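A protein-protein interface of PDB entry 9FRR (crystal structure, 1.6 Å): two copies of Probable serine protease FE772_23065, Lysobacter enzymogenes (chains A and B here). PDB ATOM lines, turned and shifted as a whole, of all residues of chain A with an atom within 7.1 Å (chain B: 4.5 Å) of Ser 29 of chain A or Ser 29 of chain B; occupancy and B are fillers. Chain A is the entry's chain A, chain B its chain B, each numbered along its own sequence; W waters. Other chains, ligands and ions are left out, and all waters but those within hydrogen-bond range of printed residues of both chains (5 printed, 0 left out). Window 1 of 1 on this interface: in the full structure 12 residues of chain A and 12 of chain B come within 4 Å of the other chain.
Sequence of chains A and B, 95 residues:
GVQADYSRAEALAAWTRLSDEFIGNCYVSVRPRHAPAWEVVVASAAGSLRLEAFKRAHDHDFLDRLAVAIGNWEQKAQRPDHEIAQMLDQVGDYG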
ATOM      1  N   PHE A  22       4.091 -21.639 -12.000  1.00  0.00           N
ATOM      2  CA  PHE A  22       3.140 -22.480 -12.709  1.00  0.00           C
ATOM      3  C   PHE A  22       3.015 -22.057 -14.170  1.00  0.00           C
ATOM      4  O   PHE A  22       2.839 -22.910 -15.048  1.00  0.00           O
ATOM      5  CB  PHE A  22       1.779 -22.443 -12.008  1.00  0.00           C
ATOM      6  CG  PHE A  22       1.664 -23.412 -10.860  1.00  0.00           C
ATOM      7  CD1 PHE A  22       2.761 -23.693 -10.056  1.00  0.00           C
ATOM      8  CD2 PHE A  22       0.462 -24.053 -10.593  1.00  0.00           C
ATOM      9  CE1 PHE A  22       2.657 -24.590  -9.003  1.00  0.00           C
ATOM     10  CE2 PHE A  22       0.353 -24.952  -9.538  1.00  0.00           C
ATOM     11  CZ  PHE A  22       1.447 -25.218  -8.747  1.00  0.00           C
ATOM     12  N   ILE A  23       3.084 -20.750 -14.451  1.00  0.00           N
ATOM     13  CA  ILE A  23       3.042 -20.299 -15.843  1.00  0.00           C
ATOM     14  C   ILE A  23       4.260 -20.814 -16.592  1.00  0.00           C
ATOM     15  O   ILE A  23       4.153 -21.303 -17.725  1.00  0.00           O
ATOM     16  CB  ILE A  23       2.937 -18.763 -15.907  1.00  0.00           C
ATOM     17  CG1 ILE A  23       1.581 -18.326 -15.360  1.00  0.00           C
ATOM     18  CG2 ILE A  23       3.152 -18.256 -17.344  1.00  0.00           C
ATOM     19  CD1 ILE A  23       1.446 -16.828 -15.193  1.00  0.00           C
ATOM     20  N   GLY A  24       5.434 -20.717 -15.966  1.00  0.00           N
ATOM     21  CA  GLY A  24       6.638 -21.256 -16.582  1.00  0.00           C
ATOM     22  C   GLY A  24       6.543 -22.746 -16.829  1.00  0.00           C
ATOM     23  O   GLY A  24       6.960 -23.239 -17.879  1.00  0.00           O
ATOM     24  N   ASN A  25       5.967 -23.488 -15.879  1.00  0.00           N
ATOM     25  CA  ASN A  25       5.803 -24.924 -16.090  1.00  0.00           C
ATOM     26  C   ASN A  25       4.883 -25.216 -17.272  1.00  0.00           C
ATOM     27  O   ASN A  25       5.154 -26.126 -18.062  1.00  0.00           O
ATOM     28  CB  ASN A  25       5.265 -25.600 -14.830  1.00  0.00           C
ATOM     29  CG  ASN A  25       6.270 -25.620 -13.707  1.00  0.00           C
ATOM     30  OD1 ASN A  25       7.459 -25.357 -13.909  1.00  0.00           O
ATOM     31  ND2 ASN A  25       5.795 -25.932 -12.501  1.00  0.00           N
ATOM     32  N   CYS A  26       3.797 -24.454 -17.419  1.00  0.00           N
ATOM     33  CA  CYS A  26       2.936 -24.599 -18.586  1.00  0.00           C
ATOM     34  C   CYS A  26       3.703 -24.316 -19.864  1.00  0.00           C
ATOM     35  O   CYS A  26       3.552 -25.031 -20.863  1.00  0.00           O
ATOM     36  CB  CYS A  26       1.762 -23.633 -18.502  1.00  0.00           C
ATOM     37  SG  CYS A  26       0.567 -24.034 -17.227  1.00  0.00           S
ATOM     38  N   TYR A  27       4.492 -23.237 -19.858  1.00  0.00           N
ATOM     39  CA  TYR A  27       5.221 -22.839 -21.055  1.00  0.00           C
ATOM     40  C   TYR A  27       6.205 -23.925 -21.469  1.00  0.00           C
ATOM     41  O   TYR A  27       6.293 -24.272 -22.655  1.00  0.00           O
ATOM     42  CB  TYR A  27       5.939 -21.508 -20.802  1.00  0.00           C
ATOM     43  CG  TYR A  27       6.615 -20.933 -22.034  1.00  0.00           C
ATOM     44  CD1 TYR A  27       7.859 -21.400 -22.450  1.00  0.00           C
ATOM     45  CD2 TYR A  27       6.008 -19.937 -22.782  1.00  0.00           C
ATOM     46  CE1 TYR A  27       8.481 -20.894 -23.582  1.00  0.00           C
ATOM     47  CE2 TYR A  27       6.633 -19.414 -23.932  1.00  0.00           C
ATOM     48  CZ  TYR A  27       7.865 -19.905 -24.314  1.00  0.00           C
ATOM     49  OH  TYR A  27       8.474 -19.397 -25.438  1.00  0.00           O
ATOM     50  N   VAL A  28       6.936 -24.486 -20.504  1.00  0.00           N
ATOM     51  CA  VAL A  28       7.884 -25.557 -20.827  1.00  0.00           C
ATOM     52  C   VAL A  28       7.168 -26.714 -21.498  1.00  0.00           C
ATOM     53  O   VAL A  28       7.666 -27.294 -22.475  1.00  0.00           O
ATOM     54  CB  VAL A  28       8.627 -26.025 -19.568  1.00  0.00           C
ATOM     55  CG1 VAL A  28       9.473 -27.264 -19.895  1.00  0.00           C
ATOM     56  CG2 VAL A  28       9.493 -24.917 -19.034  1.00  0.00           C
ATOM     57  N   SER A  29       5.978 -27.056 -21.007  1.00  0.00           N
ATOM     58  CA  SER A  29       5.272 -28.211 -21.546  1.00  0.00           C
ATOM     59  C   SER A  29       4.791 -27.962 -22.970  1.00  0.00           C
ATOM     60  O   SER A  29       4.895 -28.846 -23.825  1.00  0.00           O
ATOM     61  CB  SER A  29       4.102 -28.569 -20.631  1.00  0.00           C
ATOM     62  OG  SER A  29       4.594 -29.280 -19.499  1.00  0.00           O
ATOM     63  N   VAL A  30       4.272 -26.767 -23.265  1.00  0.00           N
ATOM     64  CA  VAL A  30       3.600 -26.563 -24.543  1.00  0.00           C
ATOM     65  C   VAL A  30       4.493 -25.955 -25.613  1.00  0.00           C
ATOM     66  O   VAL A  30       4.109 -25.971 -26.795  1.00  0.00           O
ATOM     67  CB  VAL A  30       2.341 -25.689 -24.380  1.00  0.00           C
ATOM     68  CG1 VAL A  30       1.367 -26.353 -23.426  1.00  0.00           C
ATOM     69  CG2 VAL A  30       2.729 -24.306 -23.891  1.00  0.00           C
ATOM     70  N   ARG A  31       5.665 -25.442 -25.251  1.00  0.00           N
ATOM     71  CA  ARG A  31       6.504 -24.690 -26.186  1.00  0.00           C
ATOM     72  C   ARG A  31       6.964 -25.561 -27.350  1.00  0.00           C
ATOM     73  O   ARG A  31       7.587 -26.607 -27.119  1.00  0.00           O
ATOM     74  CB  ARG A  31       7.737 -24.131 -25.474  1.00  0.00           C
ATOM     75  CG  ARG A  31       8.913 -23.916 -26.415  1.00  0.00           C
ATOM     76  CD  ARG A  31      10.188 -23.690 -25.683  1.00  0.00           C
ATOM     77  NE  ARG A  31      10.999 -24.896 -25.494  1.00  0.00           N
ATOM     78  CZ  ARG A  31      11.909 -25.312 -26.370  1.00  0.00           C
ATOM     79  NH1 ARG A  31      12.065 -24.671 -27.525  1.00  0.00           N
ATOM     80  NH2 ARG A  31      12.650 -26.377 -26.100  1.00  0.00           N
ATOM     81  N   PRO A  32       6.708 -25.168 -28.592  1.00  0.00           N
ATOM     82  CA  PRO A  32       7.259 -25.905 -29.737  1.00  0.00           C
ATOM     83  C   PRO A  32       8.710 -25.516 -29.977  1.00  0.00           C
ATOM     84  O   PRO A  32       9.209 -24.514 -29.471  1.00  0.00           O
ATOM     85  CB  PRO A  32       6.372 -25.459 -30.897  1.00  0.00           C
ATOM     86  CG  PRO A  32       6.000 -24.045 -30.527  1.00  0.00           C
ATOM     87  CD  PRO A  32       5.858 -24.042 -29.013  1.00  0.00           C
ATOM     88  N   ARG A  65      -2.733 -23.146 -27.183  1.00  0.00           N
ATOM     89  CA  ARG A  65      -2.339 -24.303 -26.386  1.00  0.00           C
ATOM     90  C   ARG A  65      -1.850 -23.882 -25.006  1.00  0.00           C
ATOM     91  O   ARG A  65      -2.104 -24.576 -24.015  1.00  0.00           O
ATOM     92  CB  ARG A  65      -1.271 -25.108 -27.125  1.00  0.00           C
ATOM     93  CG  ARG A  65      -1.747 -25.620 -28.472  1.00  0.00           C
ATOM     94  CD  ARG A  65      -0.984 -26.862 -28.897  1.00  0.00           C
ATOM     95  NE  ARG A  65       0.421 -26.786 -28.518  1.00  0.00           N
ATOM     96  CZ  ARG A  65       1.364 -26.233 -29.267  1.00  0.00           C
ATOM     97  NH1 ARG A  65       2.617 -26.210 -28.841  1.00  0.00           N
ATOM     98  NH2 ARG A  65       1.052 -25.710 -30.446  1.00  0.00           N
ATOM     99  N   LEU A  66      -1.151 -22.749 -24.918  1.00  0.00           N
ATOM    100  CA  LEU A  66      -0.742 -22.255 -23.610  1.00  0.00           C
ATOM    101  C   LEU A  66      -1.961 -21.856 -22.780  1.00  0.00           C
ATOM    102  O   LEU A  66      -2.017 -22.137 -21.580  1.00  0.00           O
ATOM    103  CB  LEU A  66       0.227 -21.078 -23.777  1.00  0.00           C
ATOM    104  CG  LEU A  66       0.824 -20.462 -22.509  1.00  0.00           C
ATOM    105  CD1 LEU A  66       1.306 -21.548 -21.538  1.00  0.00           C
ATOM    106  CD2 LEU A  66       1.987 -19.552 -22.887  1.00  0.00           C
ATOM    107  N   ALA A  67      -2.957 -21.223 -23.411  1.00  0.00           N
ATOM    108  CA  ALA A  67      -4.178 -20.859 -22.697  1.00  0.00           C
ATOM    109  C   ALA A  67      -4.889 -22.089 -22.145  1.00  0.00           C
ATOM    110  O   ALA A  67      -5.401 -22.065 -21.019  1.00  0.00           O
ATOM    111  CB  ALA A  67      -5.110 -20.068 -23.619  1.00  0.00           C
ATOM    112  N   VAL A  68      -4.926 -23.178 -22.915  1.00  0.00           N
ATOM    113  CA  VAL A  68      -5.548 -24.408 -22.423  1.00  0.00           C
ATOM    114  C   VAL A  68      -4.799 -24.927 -21.201  1.00  0.00           C
ATOM    115  O   VAL A  68      -5.411 -25.338 -20.208  1.00  0.00           O
ATOM    116  CB  VAL A  68      -5.614 -25.462 -23.544  1.00  0.00           C
ATOM    117  CG1 VAL A  68      -5.917 -26.859 -22.974  1.00  0.00           C
ATOM    118  CG2 VAL A  68      -6.649 -25.066 -24.579  1.00  0.00           C
ATOM    119  N   ALA A  69      -3.463 -24.902 -21.248  1.00  0.00           N
ATOM    120  CA  ALA A  69      -2.665 -25.345 -20.109  1.00  0.00           C
ATOM    121  C   ALA A  69      -2.965 -24.497 -18.883  1.00  0.00           C
ATOM    122  O   ALA A  69      -3.172 -25.022 -17.784  1.00  0.00           O
ATOM    123  CB  ALA A  69      -1.173 -25.282 -20.457  1.00  0.00           C
ATOM    124  N   ILE A  70      -2.982 -23.172 -19.063  1.00  0.00           N
ATOM    125  CA  ILE A  70      -3.296 -22.260 -17.970  1.00  0.00           C
ATOM    126  C   ILE A  70      -4.663 -22.595 -17.390  1.00  0.00           C
ATOM    127  O   ILE A  70      -4.824 -22.753 -16.173  1.00  0.00           O
ATOM    128  CB  ILE A  70      -3.242 -20.805 -18.471  1.00  0.00           C
ATOM    129  CG1 ILE A  70      -1.829 -20.426 -18.922  1.00  0.00           C
ATOM    130  CG2 ILE A  70      -3.793 -19.844 -17.421  1.00  0.00           C
ATOM    131  CD1 ILE A  70      -0.859 -20.315 -17.810  1.00  0.00           C
ATOM    132  N   ASN A  72      -6.260 -25.370 -17.471  1.00  0.00           N
ATOM    133  CA  ASN A  72      -6.269 -26.666 -16.802  1.00  0.00           C
ATOM    134  C   ASN A  72      -5.747 -26.559 -15.380  1.00  0.00           C
ATOM    135  O   ASN A  72      -6.293 -27.185 -14.466  1.00  0.00           O
ATOM    136  CB  ASN A  72      -5.427 -27.671 -17.582  1.00  0.00           C
ATOM    137  CG  ASN A  72      -6.142 -28.217 -18.787  1.00  0.00           C
ATOM    138  OD1 ASN A  72      -7.375 -28.186 -18.867  1.00  0.00           O
ATOM    139  ND2 ASN A  72      -5.375 -28.753 -19.726  1.00  0.00           N
ATOM    140  N   TRP A  73      -4.688 -25.775 -15.171  1.00  0.00           N
ATOM    141  CA  TRP A  73      -4.193 -25.597 -13.811  1.00  0.00           C
ATOM    142  C   TRP A  73      -5.129 -24.721 -12.992  1.00  0.00           C
ATOM    143  O   TRP A  73      -5.302 -24.961 -11.792  1.00  0.00           O
ATOM    144  CB  TRP A  73      -2.773 -25.030 -13.839  1.00  0.00           C
ATOM    145  CG  TRP A  73      -1.795 -26.083 -14.270  1.00  0.00           C
ATOM    146  CD1 TRP A  73      -1.263 -26.252 -15.516  1.00  0.00           C
ATOM    147  CD2 TRP A  73      -1.279 -27.148 -13.464  1.00  0.00           C
ATOM    148  NE1 TRP A  73      -0.432 -27.349 -15.530  1.00  0.00           N
ATOM    149  CE2 TRP A  73      -0.423 -27.911 -14.279  1.00  0.00           C
ATOM    150  CE3 TRP A  73      -1.457 -27.525 -12.128  1.00  0.00           C
ATOM    151  CZ2 TRP A  73       0.255 -29.029 -13.805  1.00  0.00           C
ATOM    152  CZ3 TRP A  73      -0.784 -28.638 -11.657  1.00  0.00           C
ATOM    153  CH2 TRP A  73       0.065 -29.373 -12.493  1.00  0.00           C
ATOM    154  N   ASN B  25       2.334 -33.779 -14.499  1.00  0.00           N
ATOM    155  CA  ASN B  25       2.309 -32.334 -14.706  1.00  0.00           C
ATOM    156  C   ASN B  25       2.251 -31.984 -16.188  1.00  0.00           C
ATOM    157  O   ASN B  25       1.531 -31.063 -16.583  1.00  0.00           O
ATOM    158  CB  ASN B  25       3.522 -31.683 -14.041  1.00  0.00           C
ATOM    159  CG  ASN B  25       3.448 -31.733 -12.532  1.00  0.00           C
ATOM    160  OD1 ASN B  25       2.404 -32.057 -11.957  1.00  0.00           O
ATOM    161  ND2 ASN B  25       4.564 -31.426 -11.877  1.00  0.00           N
ATOM    162  N   CYS B  26       2.977 -32.734 -17.030  1.00  0.00           N
ATOM    163  CA  CYS B  26       2.877 -32.563 -18.473  1.00  0.00           C
ATOM    164  C   CYS B  26       1.463 -32.834 -18.955  1.00  0.00           C
ATOM    165  O   CYS B  26       0.914 -32.079 -19.764  1.00  0.00           O
ATOM    166  CB  CYS B  26       3.830 -33.514 -19.188  1.00  0.00           C
ATOM    167  SG  CYS B  26       5.570 -33.090 -18.976  1.00  0.00           S
ATOM    168  N   TYR B  27       0.880 -33.941 -18.487  1.00  0.00           N
ATOM    169  CA  TYR B  27      -0.459 -34.324 -18.913  1.00  0.00           C
ATOM    170  C   TYR B  27      -1.471 -33.240 -18.568  1.00  0.00           C
ATOM    171  O   TYR B  27      -2.317 -32.878 -19.397  1.00  0.00           O
ATOM    172  CB  TYR B  27      -0.827 -35.660 -18.256  1.00  0.00           C
ATOM    173  CG  TYR B  27      -2.135 -36.241 -18.745  1.00  0.00           C
ATOM    174  CD1 TYR B  27      -3.349 -35.776 -18.249  1.00  0.00           C
ATOM    175  CD2 TYR B  27      -2.157 -37.259 -19.691  1.00  0.00           C
ATOM    176  CE1 TYR B  27      -4.546 -36.299 -18.690  1.00  0.00           C
ATOM    177  CE2 TYR B  27      -3.354 -37.793 -20.139  1.00  0.00           C
ATOM    178  CZ  TYR B  27      -4.547 -37.298 -19.635  1.00  0.00           C
ATOM    179  OH  TYR B  27      -5.747 -37.821 -20.073  1.00  0.00           O
ATOM    180  N   VAL B  28      -1.403 -32.713 -17.344  1.00  0.00           N
ATOM    181  CA  VAL B  28      -2.346 -31.669 -16.941  1.00  0.00           C
ATOM    182  C   VAL B  28      -2.266 -30.485 -17.895  1.00  0.00           C
ATOM    183  O   VAL B  28      -3.295 -29.896 -18.260  1.00  0.00           O
ATOM    184  CB  VAL B  28      -2.089 -31.236 -15.485  1.00  0.00           C
ATOM    185  CG1 VAL B  28      -2.895 -29.958 -15.152  1.00  0.00           C
ATOM    186  CG2 VAL B  28      -2.444 -32.343 -14.525  1.00  0.00           C
ATOM    187  N   SER B  29      -1.050 -30.121 -18.323  1.00  0.00           N
ATOM    188  CA  SER B  29      -0.907 -28.952 -19.181  1.00  0.00           C
ATOM    189  C   SER B  29      -1.475 -29.191 -20.574  1.00  0.00           C
ATOM    190  O   SER B  29      -2.148 -28.313 -21.124  1.00  0.00           O
ATOM    191  CB  SER B  29       0.558 -28.530 -19.269  1.00  0.00           C
ATOM    192  OG  SER B  29       0.956 -27.903 -18.059  1.00  0.00           O
ATOM    193  N   VAL B  30      -1.224 -30.363 -21.169  1.00  0.00           N
ATOM    194  CA  VAL B  30      -1.538 -30.552 -22.583  1.00  0.00           C
ATOM    195  C   VAL B  30      -2.905 -31.182 -22.811  1.00  0.00           C
ATOM    196  O   VAL B  30      -3.385 -31.170 -23.955  1.00  0.00           O
ATOM    197  CB  VAL B  30      -0.459 -31.391 -23.310  1.00  0.00           C
ATOM    198  CG1 VAL B  30       0.917 -30.711 -23.192  1.00  0.00           C
ATOM    199  CG2 VAL B  30      -0.409 -32.806 -22.756  1.00  0.00           C
ATOM    200  N   ARG B  31      -3.556 -31.685 -21.762  1.00  0.00           N
ATOM    201  CA  ARG B  31      -4.829 -32.405 -21.878  1.00  0.00           C
ATOM    202  C   ARG B  31      -5.922 -31.540 -22.510  1.00  0.00           C
ATOM    203  O   ARG B  31      -6.267 -30.487 -21.952  1.00  0.00           O
ATOM    204  CB  ARG B  31      -5.289 -32.853 -20.486  1.00  0.00           C
ATOM    205  CG  ARG B  31      -6.733 -33.335 -20.463  1.00  0.00           C
ATOM    206  CD  ARG B  31      -7.218 -33.521 -19.063  1.00  0.00           C
ATOM    207  NE  ARG B  31      -7.705 -32.278 -18.483  1.00  0.00           N
ATOM    208  CZ  ARG B  31      -8.949 -31.841 -18.620  1.00  0.00           C
ATOM    209  NH1 ARG B  31      -9.820 -32.544 -19.341  1.00  0.00           N
ATOM    210  NH2 ARG B  31      -9.320 -30.712 -18.029  1.00  0.00           N
ATOM    211  N   VAL B  68       6.032 -33.947 -26.945  1.00  0.00           N
ATOM    212  CA  VAL B  68       6.824 -32.720 -26.993  1.00  0.00           C
ATOM    213  C   VAL B  68       7.042 -32.178 -25.588  1.00  0.00           C
ATOM    214  O   VAL B  68       8.146 -31.743 -25.238  1.00  0.00           O
ATOM    215  CB  VAL B  68       6.142 -31.675 -27.900  1.00  0.00           C
ATOM    216  CG1 VAL B  68       6.705 -30.265 -27.654  1.00  0.00           C
ATOM    217  CG2 VAL B  68       6.325 -32.054 -29.352  1.00  0.00           C
ATOM    218  N   ALA B  69       5.998 -32.210 -24.753  1.00  0.00           N
ATOM    219  CA  ALA B  69       6.143 -31.740 -23.376  1.00  0.00           C
ATOM    220  C   ALA B  69       7.172 -32.565 -22.621  1.00  0.00           C
ATOM    221  O   ALA B  69       8.057 -32.022 -21.945  1.00  0.00           O
ATOM    222  CB  ALA B  69       4.791 -31.797 -22.663  1.00  0.00           C
ATOM    223  N   ASN B  72      10.591 -31.721 -23.718  1.00  0.00           N
ATOM    224  CA  ASN B  72      11.060 -30.434 -23.218  1.00  0.00           C
ATOM    225  C   ASN B  72      11.585 -30.557 -21.797  1.00  0.00           C
ATOM    226  O   ASN B  72      12.603 -29.943 -21.449  1.00  0.00           O
ATOM    227  CB  ASN B  72       9.941 -29.388 -23.281  1.00  0.00           C
ATOM    228  CG  ASN B  72       9.676 -28.888 -24.691  1.00  0.00           C
ATOM    229  OD1 ASN B  72      10.520 -29.009 -25.584  1.00  0.00           O
ATOM    230  ND2 ASN B  72       8.490 -28.307 -24.894  1.00  0.00           N
ATOM    231  N   TRP B  73      10.910 -31.341 -20.958  1.00  0.00           N
ATOM    232  CA  TRP B  73      11.396 -31.515 -19.596  1.00  0.00           C
ATOM    233  C   TRP B  73      12.650 -32.377 -19.571  1.00  0.00           C
ATOM    234  O   TRP B  73      13.565 -32.124 -18.779  1.00  0.00           O
ATOM    235  CB  TRP B  73      10.291 -32.093 -18.714  1.00  0.00           C
ATOM    236  CG  TRP B  73       9.261 -31.044 -18.386  1.00  0.00           C
ATOM    237  CD1 TRP B  73       8.054 -30.870 -18.988  1.00  0.00           C
ATOM    238  CD2 TRP B  73       9.390 -29.990 -17.422  1.00  0.00           C
ATOM    239  NE1 TRP B  73       7.399 -29.786 -18.435  1.00  0.00           N
ATOM    240  CE2 TRP B  73       8.201 -29.234 -17.469  1.00  0.00           C
ATOM    241  CE3 TRP B  73      10.395 -29.615 -16.521  1.00  0.00           C
ATOM    242  CZ2 TRP B  73       7.988 -28.130 -16.651  1.00  0.00           C
ATOM    243  CZ3 TRP B  73      10.182 -28.516 -15.706  1.00  0.00           C
ATOM    244  CH2 TRP B  73       8.987 -27.787 -15.777  1.00  0.00           C
HETATM  245  O   HOH W   1      -8.607 -29.083 -21.156  1.00  0.00           O
HETATM  246  O   HOH W   2       3.364 -28.623 -17.324  1.00  0.00           O
HETATM  247  O   HOH W   3       9.905 -27.982 -28.084  1.00  0.00           O
HETATM  248  O   HOH W   4      -2.505 -27.308 -23.877  1.00  0.00           O
HETATM  249  O   HOH W   5      13.014 -27.532 -22.910  1.00  0.00           O
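O of Val 28 of chain A sits at hydrogen-bond distance from ND2 of Asn 72 of chain B. The indole nitrogen (NE1) of Trp 73 of chain B sits at hydrogen-bond distance from the side-chain hydroxyl (OG) of Ser 29 of chain A (3.0 Å). The backbone carbonyl oxygen of Arg 31 of chain A is in hydrogen-bond range of the side-chain amide nitrogen of Asn 72 of chain B (2.9 Å). ND2 of Asn 72 of chain A is in hydrogen-bond range of O of Val 28 of chain B (2.8 Å). The side-chain amide nitrogen (ND2) of Asn 72 of chain A lies within hydrogen-bond range of the backbone carbonyl oxygen (O) of Arg 31 of chain B (3.0 Å). NE1 of Trp 73 of chain A sits at hydrogen-bond distance from OG of Ser 29 of chain B, at 2.9 Å.
O of Phe 22 of chain A is in hydrogen-bond range of SG of Cys 26 of chain A (3.3 Å). ND2 of Asn 72 of chain A sits close to O of Val 68 of chain A (3.4 Å). The backbone carbonyl oxygen of Val 68 of chain B sits close to the side-chain amide nitrogen of Asn 72 of chain B, 3.5 Å away.
Among the printed residues, merely in contact across the chains: Ser 29 of chain A with Ala 69 of chain B (3.2 Å), Ala 69 of chain A with Ser 29 of chain B (3.2 Å), Trp 73 of chain A with Val 28 of chain B (3.3 Å), Val 28 of chain A with Trp 73 of chain B (3.4 Å), Asn 25 of chain A with Trp 73 of chain B (3.4 Å), Asn 72 of chain A with Ser 29 of chain B (3.5 Å), Trp 73 of chain A with Asn 25 of chain B (3.6 Å), Val 68 of chain A with Arg 31 of chain B (3.8 Å), Ser 29 of chain A with Asn 72 of chain B (3.8 Å), Ser 29 of chain A with Ser 29 of chain B (3.8 Å), Arg 31 of chain A with Val 68 of chain B (3.8 Å), Ser 29 of chain A with Cys 26 of chain B (3.8 Å) and Cys 26 of chain A with Ser 29 of chain B (3.9 Å).
Ser 29 of chain B touches five residues of chain A. Printed residues of chain B within 4 Å of Val 28 of chain A: Asn 72 and Trp 73. Of the printed residues of chain B, Ala 69 of chain A touches Ser 29. Printed residues of chain B within 4 Å of Arg 31 of chain A: Val 68 (3.8 Å) and Asn 72 (2.9 Å). Tyr 27 of chain A touches none of the printed residues of chain B. Leu 66 of chain A touches none of the printed residues of chain B. The nearest residue of chain B that does not touch Ser 29 of chain A is Val 68 of chain B (4.3 Å). The nearest residue of chain A that does not touch Ser 29 of chain B is Val 68 of chain A (4.3 Å).
Hydrophobic or aromatic side chains of chain A that line the printed part of chain B: Val 28, Val 68, Ala 69 and Trp 73. Of the 11 printed residues of chain B, 9 touch a printed residue of chain A. Printed residues of chain B that touch a printed residue of chain A: Asn 25, Cys 26, Val 28, Ser 29, Arg 31, Val 68, Ala 69, Asn 72 and Trp 73. Hydrophobic or aromatic side chains of chain B within 4 Å of the printed part of chain A: Val 28, Val 68, Ala 69 and Trp 73.
Asn 25 of chain A touches Trp 73 of chain B, and with the chains exchanged Trp 73 of chain A touches Asn 25 of chain B. Ser 29 of chain A touches Ala 69 of chain B, and with the chains exchanged Ala 69 of chain A touches Ser 29 of chain B. Ser 29 of chain A touches Asn 72 of chain B, and with the chains exchanged Asn 72 of chain A touches Ser 29 of chain B. Arg 31 of chain A touches Val 68 of chain B, and with the chains exchanged Val 68 of chain A touches Arg 31 of chain B. Of the 19 pairs that touch across the chains among the printed residues, 19 have their exchanged pair printed and touching as well.
Water W2 lies within hydrogen-bond range of OG of Ser 29 of chain A, OG of Ser 29 of chain B, O of Asn 25 of chain B and O of Asn 25 of chain A. Water W1 lies within hydrogen-bond range of OD1 of Asn 72 of chain A and O of Arg 31 of chain B. Water W4 bridges the backbone carbonyl oxygen (O) of Arg 65 of chain A and the backbone carbonyl oxygen (O) of Ser 29 of chain B. Water W3 bridges OD1 of Asn 72 of chain B (2.8 Å) and O of Arg 31 of chain A (2.9 Å). Water W5 bridges O of Asn 72 of chain B (2.8 Å) and NH2 of Arg 31 of chain A (3.4 Å).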
